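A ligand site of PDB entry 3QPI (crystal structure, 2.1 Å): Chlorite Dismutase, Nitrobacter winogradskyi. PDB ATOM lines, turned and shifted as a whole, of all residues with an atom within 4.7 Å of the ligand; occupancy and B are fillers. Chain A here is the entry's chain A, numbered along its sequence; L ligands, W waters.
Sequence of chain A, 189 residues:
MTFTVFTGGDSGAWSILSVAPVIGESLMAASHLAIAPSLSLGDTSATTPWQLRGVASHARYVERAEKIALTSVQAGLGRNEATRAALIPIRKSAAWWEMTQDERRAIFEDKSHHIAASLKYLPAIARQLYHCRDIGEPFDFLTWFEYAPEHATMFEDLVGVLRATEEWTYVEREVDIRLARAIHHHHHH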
ATOM      1  N   HIS A  58      18.086   7.468 -18.847  1.00  0.00           N
ATOM      2  CA  HIS A  58      16.989   7.670 -19.805  1.00  0.00           C
ATOM      3  C   HIS A  58      16.545   9.147 -19.764  1.00  0.00           C
ATOM      4  O   HIS A  58      16.897   9.879 -18.840  1.00  0.00           O
ATOM      5  CB  HIS A  58      15.805   6.781 -19.449  1.00  0.00           C
ATOM      6  CG  HIS A  58      15.197   7.115 -18.115  1.00  0.00           C
ATOM      7  ND1 HIS A  58      15.771   6.732 -16.925  1.00  0.00           N
ATOM      8  CD2 HIS A  58      14.095   7.831 -17.789  1.00  0.00           C
ATOM      9  CE1 HIS A  58      15.048   7.192 -15.912  1.00  0.00           C
ATOM     10  NE2 HIS A  58      14.021   7.850 -16.417  1.00  0.00           N
ATOM     11  N   ALA A  59      15.777   9.562 -20.764  1.00  0.00           N
ATOM     12  CA  ALA A  59      15.335  10.963 -20.869  1.00  0.00           C
ATOM     13  C   ALA A  59      14.346  11.354 -19.767  1.00  0.00           C
ATOM     14  O   ALA A  59      13.380  10.622 -19.486  1.00  0.00           O
ATOM     15  CB  ALA A  59      14.719  11.187 -22.227  1.00  0.00           C
ATOM     16  N   ARG A  60      14.607  12.483 -19.119  1.00  0.00           N
ATOM     17  CA  ARG A  60      13.716  13.022 -18.094  1.00  0.00           C
ATOM     18  C   ARG A  60      12.794  14.124 -18.638  1.00  0.00           C
ATOM     19  O   ARG A  60      11.725  14.346 -18.098  1.00  0.00           O
ATOM     20  CB  ARG A  60      14.541  13.596 -16.940  1.00  0.00           C
ATOM     21  CG  ARG A  60      15.696  12.680 -16.489  1.00  0.00           C
ATOM     22  CD  ARG A  60      15.165  11.401 -15.838  1.00  0.00           C
ATOM     23  NE  ARG A  60      16.039  10.897 -14.779  1.00  0.00           N
ATOM     24  CZ  ARG A  60      17.025  10.044 -14.993  1.00  0.00           C
ATOM     25  NH1 ARG A  60      17.247   9.610 -16.235  1.00  0.00           N
ATOM     26  NH2 ARG A  60      17.786   9.625 -13.987  1.00  0.00           N
ATOM     27  N   TYR A  61      13.216  14.806 -19.707  1.00  0.00           N
ATOM     28  CA  TYR A  61      12.432  15.924 -20.240  1.00  0.00           C
ATOM     29  C   TYR A  61      12.184  15.839 -21.744  1.00  0.00           C
ATOM     30  O   TYR A  61      11.152  16.296 -22.225  1.00  0.00           O
ATOM     31  CB  TYR A  61      13.073  17.264 -19.879  1.00  0.00           C
ATOM     32  CG  TYR A  61      13.130  17.473 -18.382  1.00  0.00           C
ATOM     33  CD1 TYR A  61      14.335  17.362 -17.693  1.00  0.00           C
ATOM     34  CD2 TYR A  61      11.968  17.706 -17.643  1.00  0.00           C
ATOM     35  CE1 TYR A  61      14.398  17.518 -16.323  1.00  0.00           C
ATOM     36  CE2 TYR A  61      12.009  17.850 -16.256  1.00  0.00           C
ATOM     37  CZ  TYR A  61      13.241  17.765 -15.604  1.00  0.00           C
ATOM     38  OH  TYR A  61      13.350  17.909 -14.252  1.00  0.00           O
ATOM     39  N   VAL A  62      13.110  15.228 -22.480  1.00  0.00           N
ATOM     40  CA  VAL A  62      13.023  15.222 -23.941  1.00  0.00           C
ATOM     41  C   VAL A  62      11.757  14.549 -24.456  1.00  0.00           C
ATOM     42  O   VAL A  62      11.411  13.436 -24.071  1.00  0.00           O
ATOM     43  CB  VAL A  62      14.257  14.534 -24.599  1.00  0.00           C
ATOM     44  CG1 VAL A  62      13.937  14.062 -26.039  1.00  0.00           C
ATOM     45  CG2 VAL A  62      15.411  15.482 -24.614  1.00  0.00           C
ATOM     46  N   LEU A  70      17.319  16.548 -32.198  1.00  0.00           N
ATOM     47  CA  LEU A  70      18.651  16.393 -31.636  1.00  0.00           C
ATOM     48  C   LEU A  70      19.472  15.366 -32.400  1.00  0.00           C
ATOM     49  O   LEU A  70      20.617  15.625 -32.770  1.00  0.00           O
ATOM     50  CB  LEU A  70      18.560  15.959 -30.173  1.00  0.00           C
ATOM     51  CG  LEU A  70      18.093  17.062 -29.213  1.00  0.00           C
ATOM     52  CD1 LEU A  70      17.510  16.468 -27.929  1.00  0.00           C
ATOM     53  CD2 LEU A  70      19.262  17.994 -28.913  1.00  0.00           C
ATOM     54  N   ILE A  88      31.470  19.879 -16.358  1.00  0.00           N
ATOM     55  CA  ILE A  88      30.788  20.828 -15.486  1.00  0.00           C
ATOM     56  C   ILE A  88      29.822  20.101 -14.537  1.00  0.00           C
ATOM     57  O   ILE A  88      28.691  19.752 -14.924  1.00  0.00           O
ATOM     58  CB  ILE A  88      30.060  21.925 -16.287  1.00  0.00           C
ATOM     59  CG1 ILE A  88      31.044  22.658 -17.212  1.00  0.00           C
ATOM     60  CG2 ILE A  88      29.366  22.929 -15.345  1.00  0.00           C
ATOM     61  CD1 ILE A  88      30.351  23.588 -18.209  1.00  0.00           C
ATOM     62  N   ILE A  90      27.193  19.838 -11.567  1.00  0.00           N
ATOM     63  CA  ILE A  90      26.119  20.761 -11.197  1.00  0.00           C
ATOM     64  C   ILE A  90      25.190  20.151 -10.129  1.00  0.00           C
ATOM     65  O   ILE A  90      24.895  18.961 -10.157  1.00  0.00           O
ATOM     66  CB  ILE A  90      25.254  21.151 -12.435  1.00  0.00           C
ATOM     67  CG1 ILE A  90      25.990  22.196 -13.284  1.00  0.00           C
ATOM     68  CG2 ILE A  90      23.847  21.681 -12.003  1.00  0.00           C
ATOM     69  CD1 ILE A  90      25.488  22.257 -14.721  1.00  0.00           C
ATOM     70  N   LYS A  92      21.457  21.117  -8.275  1.00  0.00           N
ATOM     71  CA  LYS A  92      20.296  21.989  -8.180  1.00  0.00           C
ATOM     72  C   LYS A  92      19.736  21.953  -6.744  1.00  0.00           C
ATOM     73  O   LYS A  92      20.016  21.021  -5.968  1.00  0.00           O
ATOM     74  CB  LYS A  92      19.238  21.611  -9.230  1.00  0.00           C
ATOM     75  CG  LYS A  92      19.741  21.821 -10.679  1.00  0.00           C
ATOM     76  CD  LYS A  92      18.640  21.563 -11.689  1.00  0.00           C
ATOM     77  CE  LYS A  92      19.079  21.864 -13.128  1.00  0.00           C
ATOM     78  NZ  LYS A  92      17.934  21.759 -14.081  1.00  0.00           N
ATOM     79  N   TRP A  96      14.222  23.144  -6.408  1.00  0.00           N
ATOM     80  CA  TRP A  96      14.086  22.503  -7.726  1.00  0.00           C
ATOM     81  C   TRP A  96      13.457  21.111  -7.625  1.00  0.00           C
ATOM     82  O   TRP A  96      12.492  20.770  -8.314  1.00  0.00           O
ATOM     83  CB  TRP A  96      15.462  22.373  -8.426  1.00  0.00           C
ATOM     84  CG  TRP A  96      15.376  21.633  -9.743  1.00  0.00           C
ATOM     85  CD1 TRP A  96      15.740  20.323 -10.002  1.00  0.00           C
ATOM     86  CD2 TRP A  96      14.873  22.151 -11.000  1.00  0.00           C
ATOM     87  NE1 TRP A  96      15.503  20.011 -11.326  1.00  0.00           N
ATOM     88  CE2 TRP A  96      14.979  21.108 -11.959  1.00  0.00           C
ATOM     89  CE3 TRP A  96      14.347  23.394 -11.393  1.00  0.00           C
ATOM     90  CZ2 TRP A  96      14.568  21.278 -13.286  1.00  0.00           C
ATOM     91  CZ3 TRP A  96      13.952  23.560 -12.718  1.00  0.00           C
ATOM     92  CH2 TRP A  96      14.048  22.510 -13.643  1.00  0.00           C
ATOM     93  N   PHE A 108      12.566  24.318 -17.566  1.00  0.00           N
ATOM     94  CA  PHE A 108      13.667  23.778 -18.365  1.00  0.00           C
ATOM     95  C   PHE A 108      13.531  24.177 -19.823  1.00  0.00           C
ATOM     96  O   PHE A 108      14.462  24.698 -20.415  1.00  0.00           O
ATOM     97  CB  PHE A 108      13.711  22.253 -18.216  1.00  0.00           C
ATOM     98  CG  PHE A 108      14.630  21.537 -19.195  1.00  0.00           C
ATOM     99  CD1 PHE A 108      15.984  21.344 -18.887  1.00  0.00           C
ATOM    100  CD2 PHE A 108      14.137  21.002 -20.377  1.00  0.00           C
ATOM    101  CE1 PHE A 108      16.822  20.651 -19.765  1.00  0.00           C
ATOM    102  CE2 PHE A 108      14.983  20.313 -21.261  1.00  0.00           C
ATOM    103  CZ  PHE A 108      16.317  20.143 -20.944  1.00  0.00           C
ATOM    104  N   HIS A 114      16.132  25.413 -22.925  1.00  0.00           N
ATOM    105  CA  HIS A 114      17.397  24.693 -22.830  1.00  0.00           C
ATOM    106  C   HIS A 114      17.697  23.969 -24.121  1.00  0.00           C
ATOM    107  O   HIS A 114      18.821  23.997 -24.608  1.00  0.00           O
ATOM    108  CB  HIS A 114      17.329  23.679 -21.682  1.00  0.00           C
ATOM    109  CG  HIS A 114      18.649  23.074 -21.329  1.00  0.00           C
ATOM    110  ND1 HIS A 114      19.178  23.147 -20.066  1.00  0.00           N
ATOM    111  CD2 HIS A 114      19.532  22.369 -22.075  1.00  0.00           C
ATOM    112  CE1 HIS A 114      20.339  22.518 -20.043  1.00  0.00           C
ATOM    113  NE2 HIS A 114      20.579  22.046 -21.252  1.00  0.00           N
ATOM    114  N   ILE A 115      16.691  23.303 -24.669  1.00  0.00           N
ATOM    115  CA  ILE A 115      16.918  22.527 -25.860  1.00  0.00           C
ATOM    116  C   ILE A 115      16.924  23.420 -27.074  1.00  0.00           C
ATOM    117  O   ILE A 115      17.910  23.440 -27.823  1.00  0.00           O
ATOM    118  CB  ILE A 115      15.867  21.430 -26.031  1.00  0.00           C
ATOM    119  CG1 ILE A 115      15.946  20.457 -24.846  1.00  0.00           C
ATOM    120  CG2 ILE A 115      16.104  20.656 -27.328  1.00  0.00           C
ATOM    121  CD1 ILE A 115      14.940  19.293 -24.883  1.00  0.00           C
ATOM    122  N   SER A 118      19.793  25.680 -27.638  1.00  0.00           N
ATOM    123  CA  SER A 118      21.123  25.079 -27.714  1.00  0.00           C
ATOM    124  C   SER A 118      21.368  24.365 -29.032  1.00  0.00           C
ATOM    125  O   SER A 118      22.515  24.109 -29.394  1.00  0.00           O
ATOM    126  CB  SER A 118      21.361  24.122 -26.544  1.00  0.00           C
ATOM    127  OG  SER A 118      21.324  24.824 -25.318  1.00  0.00           O
ATOM    128  N   LEU A 122      25.131  22.642 -32.155  1.00  0.00           N
ATOM    129  CA  LEU A 122      25.484  21.325 -32.689  1.00  0.00           C
ATOM    130  C   LEU A 122      25.589  21.483 -34.185  1.00  0.00           C
ATOM    131  O   LEU A 122      24.853  22.276 -34.775  1.00  0.00           O
ATOM    132  CB  LEU A 122      24.417  20.260 -32.348  1.00  0.00           C
ATOM    133  CG  LEU A 122      23.665  20.365 -31.010  1.00  0.00           C
ATOM    134  CD1 LEU A 122      22.719  19.189 -30.827  1.00  0.00           C
ATOM    135  CD2 LEU A 122      24.624  20.481 -29.819  1.00  0.00           C
ATOM    136  N   ILE A 125      29.446  21.238 -30.708  1.00  0.00           N
ATOM    137  CA  ILE A 125      29.612  20.772 -29.341  1.00  0.00           C
ATOM    138  C   ILE A 125      28.932  19.419 -29.177  1.00  0.00           C
ATOM    139  O   ILE A 125      27.731  19.329 -29.352  1.00  0.00           O
ATOM    140  CB  ILE A 125      28.997  21.771 -28.304  1.00  0.00           C
ATOM    141  CG1 ILE A 125      29.399  23.230 -28.609  1.00  0.00           C
ATOM    142  CG2 ILE A 125      29.383  21.386 -26.886  1.00  0.00           C
ATOM    143  CD1 ILE A 125      30.917  23.520 -28.514  1.00  0.00           C
ATOM    144  N   ARG A 127      28.016  16.233 -26.532  1.00  0.00           N
ATOM    145  CA  ARG A 127      27.700  16.228 -25.099  1.00  0.00           C
ATOM    146  C   ARG A 127      27.326  14.842 -24.594  1.00  0.00           C
ATOM    147  O   ARG A 127      26.839  13.993 -25.348  1.00  0.00           O
ATOM    148  CB  ARG A 127      26.526  17.177 -24.802  1.00  0.00           C
ATOM    149  CG  ARG A 127      25.199  16.654 -25.335  1.00  0.00           C
ATOM    150  CD  ARG A 127      24.027  17.610 -25.116  1.00  0.00           C
ATOM    151  NE  ARG A 127      22.782  16.864 -25.258  1.00  0.00           N
ATOM    152  CZ  ARG A 127      22.308  16.424 -26.425  1.00  0.00           C
ATOM    153  NH1 ARG A 127      22.970  16.679 -27.548  1.00  0.00           N
ATOM    154  NH2 ARG A 127      21.182  15.712 -26.484  1.00  0.00           N
ATOM    155  N   LEU A 129      25.419  13.539 -20.744  1.00  0.00           N
ATOM    156  CA  LEU A 129      24.918  13.843 -19.416  1.00  0.00           C
ATOM    157  C   LEU A 129      24.961  12.611 -18.505  1.00  0.00           C
ATOM    158  O   LEU A 129      24.498  11.538 -18.890  1.00  0.00           O
ATOM    159  CB  LEU A 129      23.460  14.316 -19.543  1.00  0.00           C
ATOM    160  CG  LEU A 129      22.695  14.584 -18.258  1.00  0.00           C
ATOM    161  CD1 LEU A 129      23.281  15.769 -17.464  1.00  0.00           C
ATOM    162  CD2 LEU A 129      21.223  14.824 -18.582  1.00  0.00           C
ATOM    163  N   PHE A 141      24.389  16.355 -11.409  1.00  0.00           N
ATOM    164  CA  PHE A 141      24.706  15.960 -12.763  1.00  0.00           C
ATOM    165  C   PHE A 141      26.197  16.143 -13.008  1.00  0.00           C
ATOM    166  O   PHE A 141      26.813  17.004 -12.395  1.00  0.00           O
ATOM    167  CB  PHE A 141      23.932  16.812 -13.774  1.00  0.00           C
ATOM    168  CG  PHE A 141      22.473  16.934 -13.472  1.00  0.00           C
ATOM    169  CD1 PHE A 141      21.604  15.897 -13.807  1.00  0.00           C
ATOM    170  CD2 PHE A 141      21.962  18.076 -12.850  1.00  0.00           C
ATOM    171  CE1 PHE A 141      20.230  16.003 -13.512  1.00  0.00           C
ATOM    172  CE2 PHE A 141      20.605  18.178 -12.553  1.00  0.00           C
ATOM    173  CZ  PHE A 141      19.738  17.143 -12.902  1.00  0.00           C
ATOM    174  N   THR A 143      28.158  16.999 -16.420  1.00  0.00           N
ATOM    175  CA  THR A 143      27.942  17.358 -17.814  1.00  0.00           C
ATOM    176  C   THR A 143      29.305  17.342 -18.494  1.00  0.00           C
ATOM    177  O   THR A 143      30.276  17.885 -17.980  1.00  0.00           O
ATOM    178  CB  THR A 143      27.185  18.712 -17.962  1.00  0.00           C
ATOM    179  OG1 THR A 143      27.928  19.796 -17.378  1.00  0.00           O
ATOM    180  CG2 THR A 143      25.820  18.629 -17.295  1.00  0.00           C
ATOM    181  N   PHE A 145      31.394  17.656 -22.254  1.00  0.00           N
ATOM    182  CA  PHE A 145      31.349  18.260 -23.575  1.00  0.00           C
ATOM    183  C   PHE A 145      32.701  18.130 -24.271  1.00  0.00           C
ATOM    184  O   PHE A 145      33.756  18.263 -23.633  1.00  0.00           O
ATOM    185  CB  PHE A 145      30.977  19.752 -23.452  1.00  0.00           C
ATOM    186  CG  PHE A 145      29.743  19.981 -22.651  1.00  0.00           C
ATOM    187  CD1 PHE A 145      28.495  19.880 -23.249  1.00  0.00           C
ATOM    188  CD2 PHE A 145      29.813  20.249 -21.288  1.00  0.00           C
ATOM    189  CE1 PHE A 145      27.359  20.036 -22.510  1.00  0.00           C
ATOM    190  CE2 PHE A 145      28.681  20.407 -20.541  1.00  0.00           C
ATOM    191  CZ  PHE A 145      27.441  20.310 -21.145  1.00  0.00           C
ATOM    192  N   PHE A 155      31.691  27.547 -27.244  1.00  0.00           N
ATOM    193  CA  PHE A 155      31.321  26.801 -26.048  1.00  0.00           C
ATOM    194  C   PHE A 155      31.169  27.717 -24.830  1.00  0.00           C
ATOM    195  O   PHE A 155      30.173  27.630 -24.120  1.00  0.00           O
ATOM    196  CB  PHE A 155      32.280  25.635 -25.737  1.00  0.00           C
ATOM    197  CG  PHE A 155      31.889  24.866 -24.496  1.00  0.00           C
ATOM    198  CD1 PHE A 155      30.798  24.003 -24.520  1.00  0.00           C
ATOM    199  CD2 PHE A 155      32.571  25.045 -23.302  1.00  0.00           C
ATOM    200  CE1 PHE A 155      30.396  23.336 -23.382  1.00  0.00           C
ATOM    201  CE2 PHE A 155      32.196  24.390 -22.173  1.00  0.00           C
ATOM    202  CZ  PHE A 155      31.100  23.526 -22.205  1.00  0.00           C
ATOM    203  N   LEU A 158      27.818  29.568 -25.252  1.00  0.00           N
ATOM    204  CA  LEU A 158      26.689  28.725 -24.883  1.00  0.00           C
ATOM    205  C   LEU A 158      26.548  28.636 -23.353  1.00  0.00           C
ATOM    206  O   LEU A 158      25.477  28.824 -22.803  1.00  0.00           O
ATOM    207  CB  LEU A 158      26.862  27.322 -25.471  1.00  0.00           C
ATOM    208  CG  LEU A 158      25.898  26.294 -24.876  1.00  0.00           C
ATOM    209  CD1 LEU A 158      24.456  26.728 -25.128  1.00  0.00           C
ATOM    210  CD2 LEU A 158      26.187  24.932 -25.466  1.00  0.00           C
ATOM    211  N   VAL A 159      27.641  28.355 -22.671  1.00  0.00           N
ATOM    212  CA  VAL A 159      27.600  28.230 -21.227  1.00  0.00           C
ATOM    213  C   VAL A 159      27.097  29.527 -20.584  1.00  0.00           C
ATOM    214  O   VAL A 159      26.251  29.503 -19.683  1.00  0.00           O
ATOM    215  CB  VAL A 159      28.994  27.861 -20.671  1.00  0.00           C
ATOM    216  CG1 VAL A 159      29.020  27.999 -19.136  1.00  0.00           C
ATOM    217  CG2 VAL A 159      29.397  26.430 -21.127  1.00  0.00           C
ATOM    218  N   LEU A 162      23.295  29.809 -21.000  1.00  0.00           N
ATOM    219  CA  LEU A 162      22.473  28.935 -20.168  1.00  0.00           C
ATOM    220  C   LEU A 162      22.517  29.418 -18.737  1.00  0.00           C
ATOM    221  O   LEU A 162      21.512  29.349 -18.026  1.00  0.00           O
ATOM    222  CB  LEU A 162      22.968  27.484 -20.250  1.00  0.00           C
ATOM    223  CG  LEU A 162      22.652  26.797 -21.580  1.00  0.00           C
ATOM    224  CD1 LEU A 162      23.411  25.486 -21.692  1.00  0.00           C
ATOM    225  CD2 LEU A 162      21.148  26.560 -21.710  1.00  0.00           C
ATOM    226  N   GLU A 167      16.184  28.472 -15.447  1.00  0.00           N
ATOM    227  CA  GLU A 167      16.648  27.176 -15.011  1.00  0.00           C
ATOM    228  C   GLU A 167      17.870  27.318 -14.094  1.00  0.00           C
ATOM    229  O   GLU A 167      17.947  26.662 -13.056  1.00  0.00           O
ATOM    230  CB  GLU A 167      16.993  26.266 -16.190  1.00  0.00           C
ATOM    231  CG  GLU A 167      17.675  24.954 -15.716  1.00  0.00           C
ATOM    232  CD  GLU A 167      17.905  23.945 -16.843  1.00  0.00           C
ATOM    233  OE1 GLU A 167      17.728  24.305 -18.017  1.00  0.00           O
ATOM    234  OE2 GLU A 167      18.242  22.778 -16.535  1.00  0.00           O
ATOM    235  N   TRP A 168      18.806  28.176 -14.470  1.00  0.00           N
ATOM    236  CA  TRP A 168      20.048  28.262 -13.716  1.00  0.00           C
ATOM    237  C   TRP A 168      19.930  28.952 -12.357  1.00  0.00           C
ATOM    238  O   TRP A 168      20.848  28.825 -11.540  1.00  0.00           O
ATOM    239  CB  TRP A 168      21.183  28.889 -14.535  1.00  0.00           C
ATOM    240  CG  TRP A 168      22.233  27.811 -14.877  1.00  0.00           C
ATOM    241  CD1 TRP A 168      23.463  27.630 -14.287  1.00  0.00           C
ATOM    242  CD2 TRP A 168      22.089  26.757 -15.846  1.00  0.00           C
ATOM    243  NE1 TRP A 168      24.099  26.540 -14.860  1.00  0.00           N
ATOM    244  CE2 TRP A 168      23.285  25.990 -15.816  1.00  0.00           C
ATOM    245  CE3 TRP A 168      21.081  26.402 -16.750  1.00  0.00           C
ATOM    246  CZ2 TRP A 168      23.487  24.893 -16.656  1.00  0.00           C
ATOM    247  CZ3 TRP A 168      21.287  25.318 -17.595  1.00  0.00           C
ATOM    248  CH2 TRP A 168      22.477  24.567 -17.527  1.00  0.00           C
ATOM    249  N   GLU A 174      28.319  24.538  -8.727  1.00  0.00           N
ATOM    250  CA  GLU A 174      28.740  24.366 -10.106  1.00  0.00           C
ATOM    251  C   GLU A 174      30.220  24.688 -10.227  1.00  0.00           C
ATOM    252  O   GLU A 174      30.683  25.686  -9.701  1.00  0.00           O
ATOM    253  CB  GLU A 174      27.929  25.282 -11.019  1.00  0.00           C
ATOM    254  CG  GLU A 174      28.285  25.208 -12.486  1.00  0.00           C
ATOM    255  CD  GLU A 174      27.279  25.956 -13.336  1.00  0.00           C
ATOM    256  OE1 GLU A 174      26.596  26.842 -12.795  1.00  0.00           O
ATOM    257  OE2 GLU A 174      27.136  25.642 -14.527  1.00  0.00           O
HETATM  258  C1  LIG L   1      19.851  18.323 -19.851  1.00  0.00           C
HETATM  259  C2  LIG L   1      20.557  19.427 -24.458  1.00  0.00           C
HETATM  260  C3  LIG L   1      24.447  22.070 -23.230  1.00  0.00           C
HETATM  261  C4  LIG L   1      23.532  21.185 -18.678  1.00  0.00           C
HETATM  262  C5  LIG L   1      19.767  18.409 -21.200  1.00  0.00           C
HETATM  263  C6  LIG L   1      18.749  17.709 -21.955  1.00  0.00           C
HETATM  264  C7  LIG L   1      18.917  17.990 -23.263  1.00  0.00           C
HETATM  265  C8  LIG L   1      20.061  18.895 -23.335  1.00  0.00           C
HETATM  266  C9  LIG L   1      18.016  17.462 -24.449  1.00  0.00           C
HETATM  267  C10 LIG L   1      17.672  16.864 -21.250  1.00  0.00           C
HETATM  268  C11 LIG L   1      17.977  15.375 -21.216  1.00  0.00           C
HETATM  269  C12 LIG L   1      16.727  14.706 -20.667  1.00  0.00           C
HETATM  270  O1  LIG L   1      16.822  14.225 -19.532  1.00  0.00           O
HETATM  271  O2  LIG L   1      15.653  14.688 -21.342  1.00  0.00           O
HETATM  272  C13 LIG L   1      21.666  20.200 -24.450  1.00  0.00           C
HETATM  273  C14 LIG L   1      22.314  20.599 -25.672  1.00  0.00           C
HETATM  274  C15 LIG L   1      23.396  21.280 -25.328  1.00  0.00           C
HETATM  275  C16 LIG L   1      23.463  21.378 -23.887  1.00  0.00           C
HETATM  276  C17 LIG L   1      21.896  20.271 -27.127  1.00  0.00           C
HETATM  277  C18 LIG L   1      24.371  21.898 -26.368  1.00  0.00           C
HETATM  278  C19 LIG L   1      25.672  21.653 -26.259  1.00  0.00           C
HETATM  279  C20 LIG L   1      24.551  22.103 -21.885  1.00  0.00           C
HETATM  280  C21 LIG L   1      25.563  22.774 -21.070  1.00  0.00           C
HETATM  281  C22 LIG L   1      25.293  22.472 -19.798  1.00  0.00           C
HETATM  282  C23 LIG L   1      24.103  21.652 -19.800  1.00  0.00           C
HETATM  283  C24 LIG L   1      26.752  23.592 -21.636  1.00  0.00           C
HETATM  284  C25 LIG L   1      25.997  22.906 -18.504  1.00  0.00           C
HETATM  285  C26 LIG L   1      26.671  24.066 -18.471  1.00  0.00           C
HETATM  286  C27 LIG L   1      22.522  20.325 -18.548  1.00  0.00           C
HETATM  287  C28 LIG L   1      22.028  19.837 -17.276  1.00  0.00           C
HETATM  288  C29 LIG L   1      20.874  18.931 -17.679  1.00  0.00           C
HETATM  289  C30 LIG L   1      20.790  19.001 -19.123  1.00  0.00           C
HETATM  290  C31 LIG L   1      22.526  20.123 -15.817  1.00  0.00           C
HETATM  291  C32 LIG L   1      19.958  18.129 -16.748  1.00  0.00           C
HETATM  292  C33 LIG L   1      18.723  19.023 -16.509  1.00  0.00           C
HETATM  293  C34 LIG L   1      17.854  18.375 -15.460  1.00  0.00           C
HETATM  294  O3  LIG L   1      17.490  17.187 -15.639  1.00  0.00           O
HETATM  295  O4  LIG L   1      17.514  19.048 -14.439  1.00  0.00           O
HETATM  296  N1  LIG L   1      20.603  19.138 -22.070  1.00  0.00           N
HETATM  297  N2  LIG L   1      22.381  20.686 -23.349  1.00  0.00           N
HETATM  298  N3  LIG L   1      23.670  21.436 -21.084  1.00  0.00           N
HETATM  299  N4  LIG L   1      21.758  19.816 -19.622  1.00  0.00           N
HETATM  300 FE1  LIG L   1      22.062  20.444 -21.401  1.00  0.00          FE
HETATM  301  O   HOH W   1      18.808  12.058 -19.119  1.00  0.00           O
HETATM  302  O   HOH W   2      15.488  17.763 -13.149  1.00  0.00           O
HETATM  303  O   HOH W   3      16.533  15.241 -13.710  1.00  0.00           O
HETATM  304  O   HOH W   4      17.870  15.106 -17.502  1.00  0.00           O
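NE2 of His 114 binds FE1 of the ligand (2.2 Å). The side-chain amino group (NZ) of Lys 92 lies within salt-bridge range of an oxygen (O4) of the ligand, at 2.8 Å. The backbone NH (N) of Val 62 lies within hydrogen-bond range of an oxygen (O2) of the ligand, 2.8 Å away. The backbone NH of Arg 60 is in hydrogen-bond range of an oxygen (O1) of the ligand (2.8 Å). The backbone NH (N) of Tyr 61 sits at hydrogen-bond distance from an oxygen (O2) of the ligand (2.9 Å).
The backbone carbonyl oxygen of Phe 108 lies within hydrogen-bond range of the backbone NH of His 114. O of His 114 is in hydrogen-bond range of OG of Ser 118, at 2.7 Å. The side-chain carboxylate of Glu 167 lies within hydrogen-bond range of a ring nitrogen (ND1) of His 114, at 2.8 Å. The side-chain amino group (NZ) of Lys 92 lies within salt-bridge range of the side-chain carboxylate (OE2) of Glu 167, 2.7 Å away. O of His 58 lies within hydrogen-bond range of NH1 of Arg 60, 2.6 Å away. The backbone NH (N) of Phe 141 lies within hydrogen-bond range of the backbone carbonyl oxygen (O) of Ile 90, at 2.9 Å. The side-chain carboxylate (OE2) of Glu 174 sits at hydrogen-bond distance from the indole nitrogen (NE1) of Trp 168. The side-chain hydroxyl (OG1) of Thr 143 sits at hydrogen-bond distance from the backbone carbonyl oxygen (O) of Ile 88 (2.6 Å).
Merely in contact with the ligand: Phe 145, Phe 141, Leu 158, Arg 127, Leu 162, Phe 108, Ile 115, Leu 70, Trp 168, Thr 143, Ser 118, Ile 88, Ala 59, Leu 122, Ile 125, Glu 167, Ile 90, Trp 96, Val 159 and Leu 129. Hydrophobic or aromatic side chains that line the ligand: Ala 59, Tyr 61, Val 62, Leu 70, Ile 88, Ile 90, Trp 96, Phe 108, His 114, Ile 115, Leu 122, Ile 125, Leu 129, Phe 141, Phe 145, Leu 158, Val 159, Leu 162 and Trp 168. 25 residues have an atom within 4 Å of the ligand: Ala 59, Arg 60, Tyr 61, Val 62, Leu 70, Ile 88, Ile 90, Lys 92, Trp 96, Phe 108, His 114, Ile 115, Ser 118, Leu 122, Ile 125, Arg 127, Leu 129, Phe 141, Thr 143, Phe 145, Leu 158, Val 159, Leu 162, Glu 167 and Trp 168.
Water W2 lies within hydrogen-bond range of OH of Tyr 61, O4 of the ligand and NE1 of Trp 96. Water W1 lies within hydrogen-bond range of the backbone carbonyl oxygen (O) of His 58 (2.9 Å) and an oxygen (O1) of the ligand (3.0 Å).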
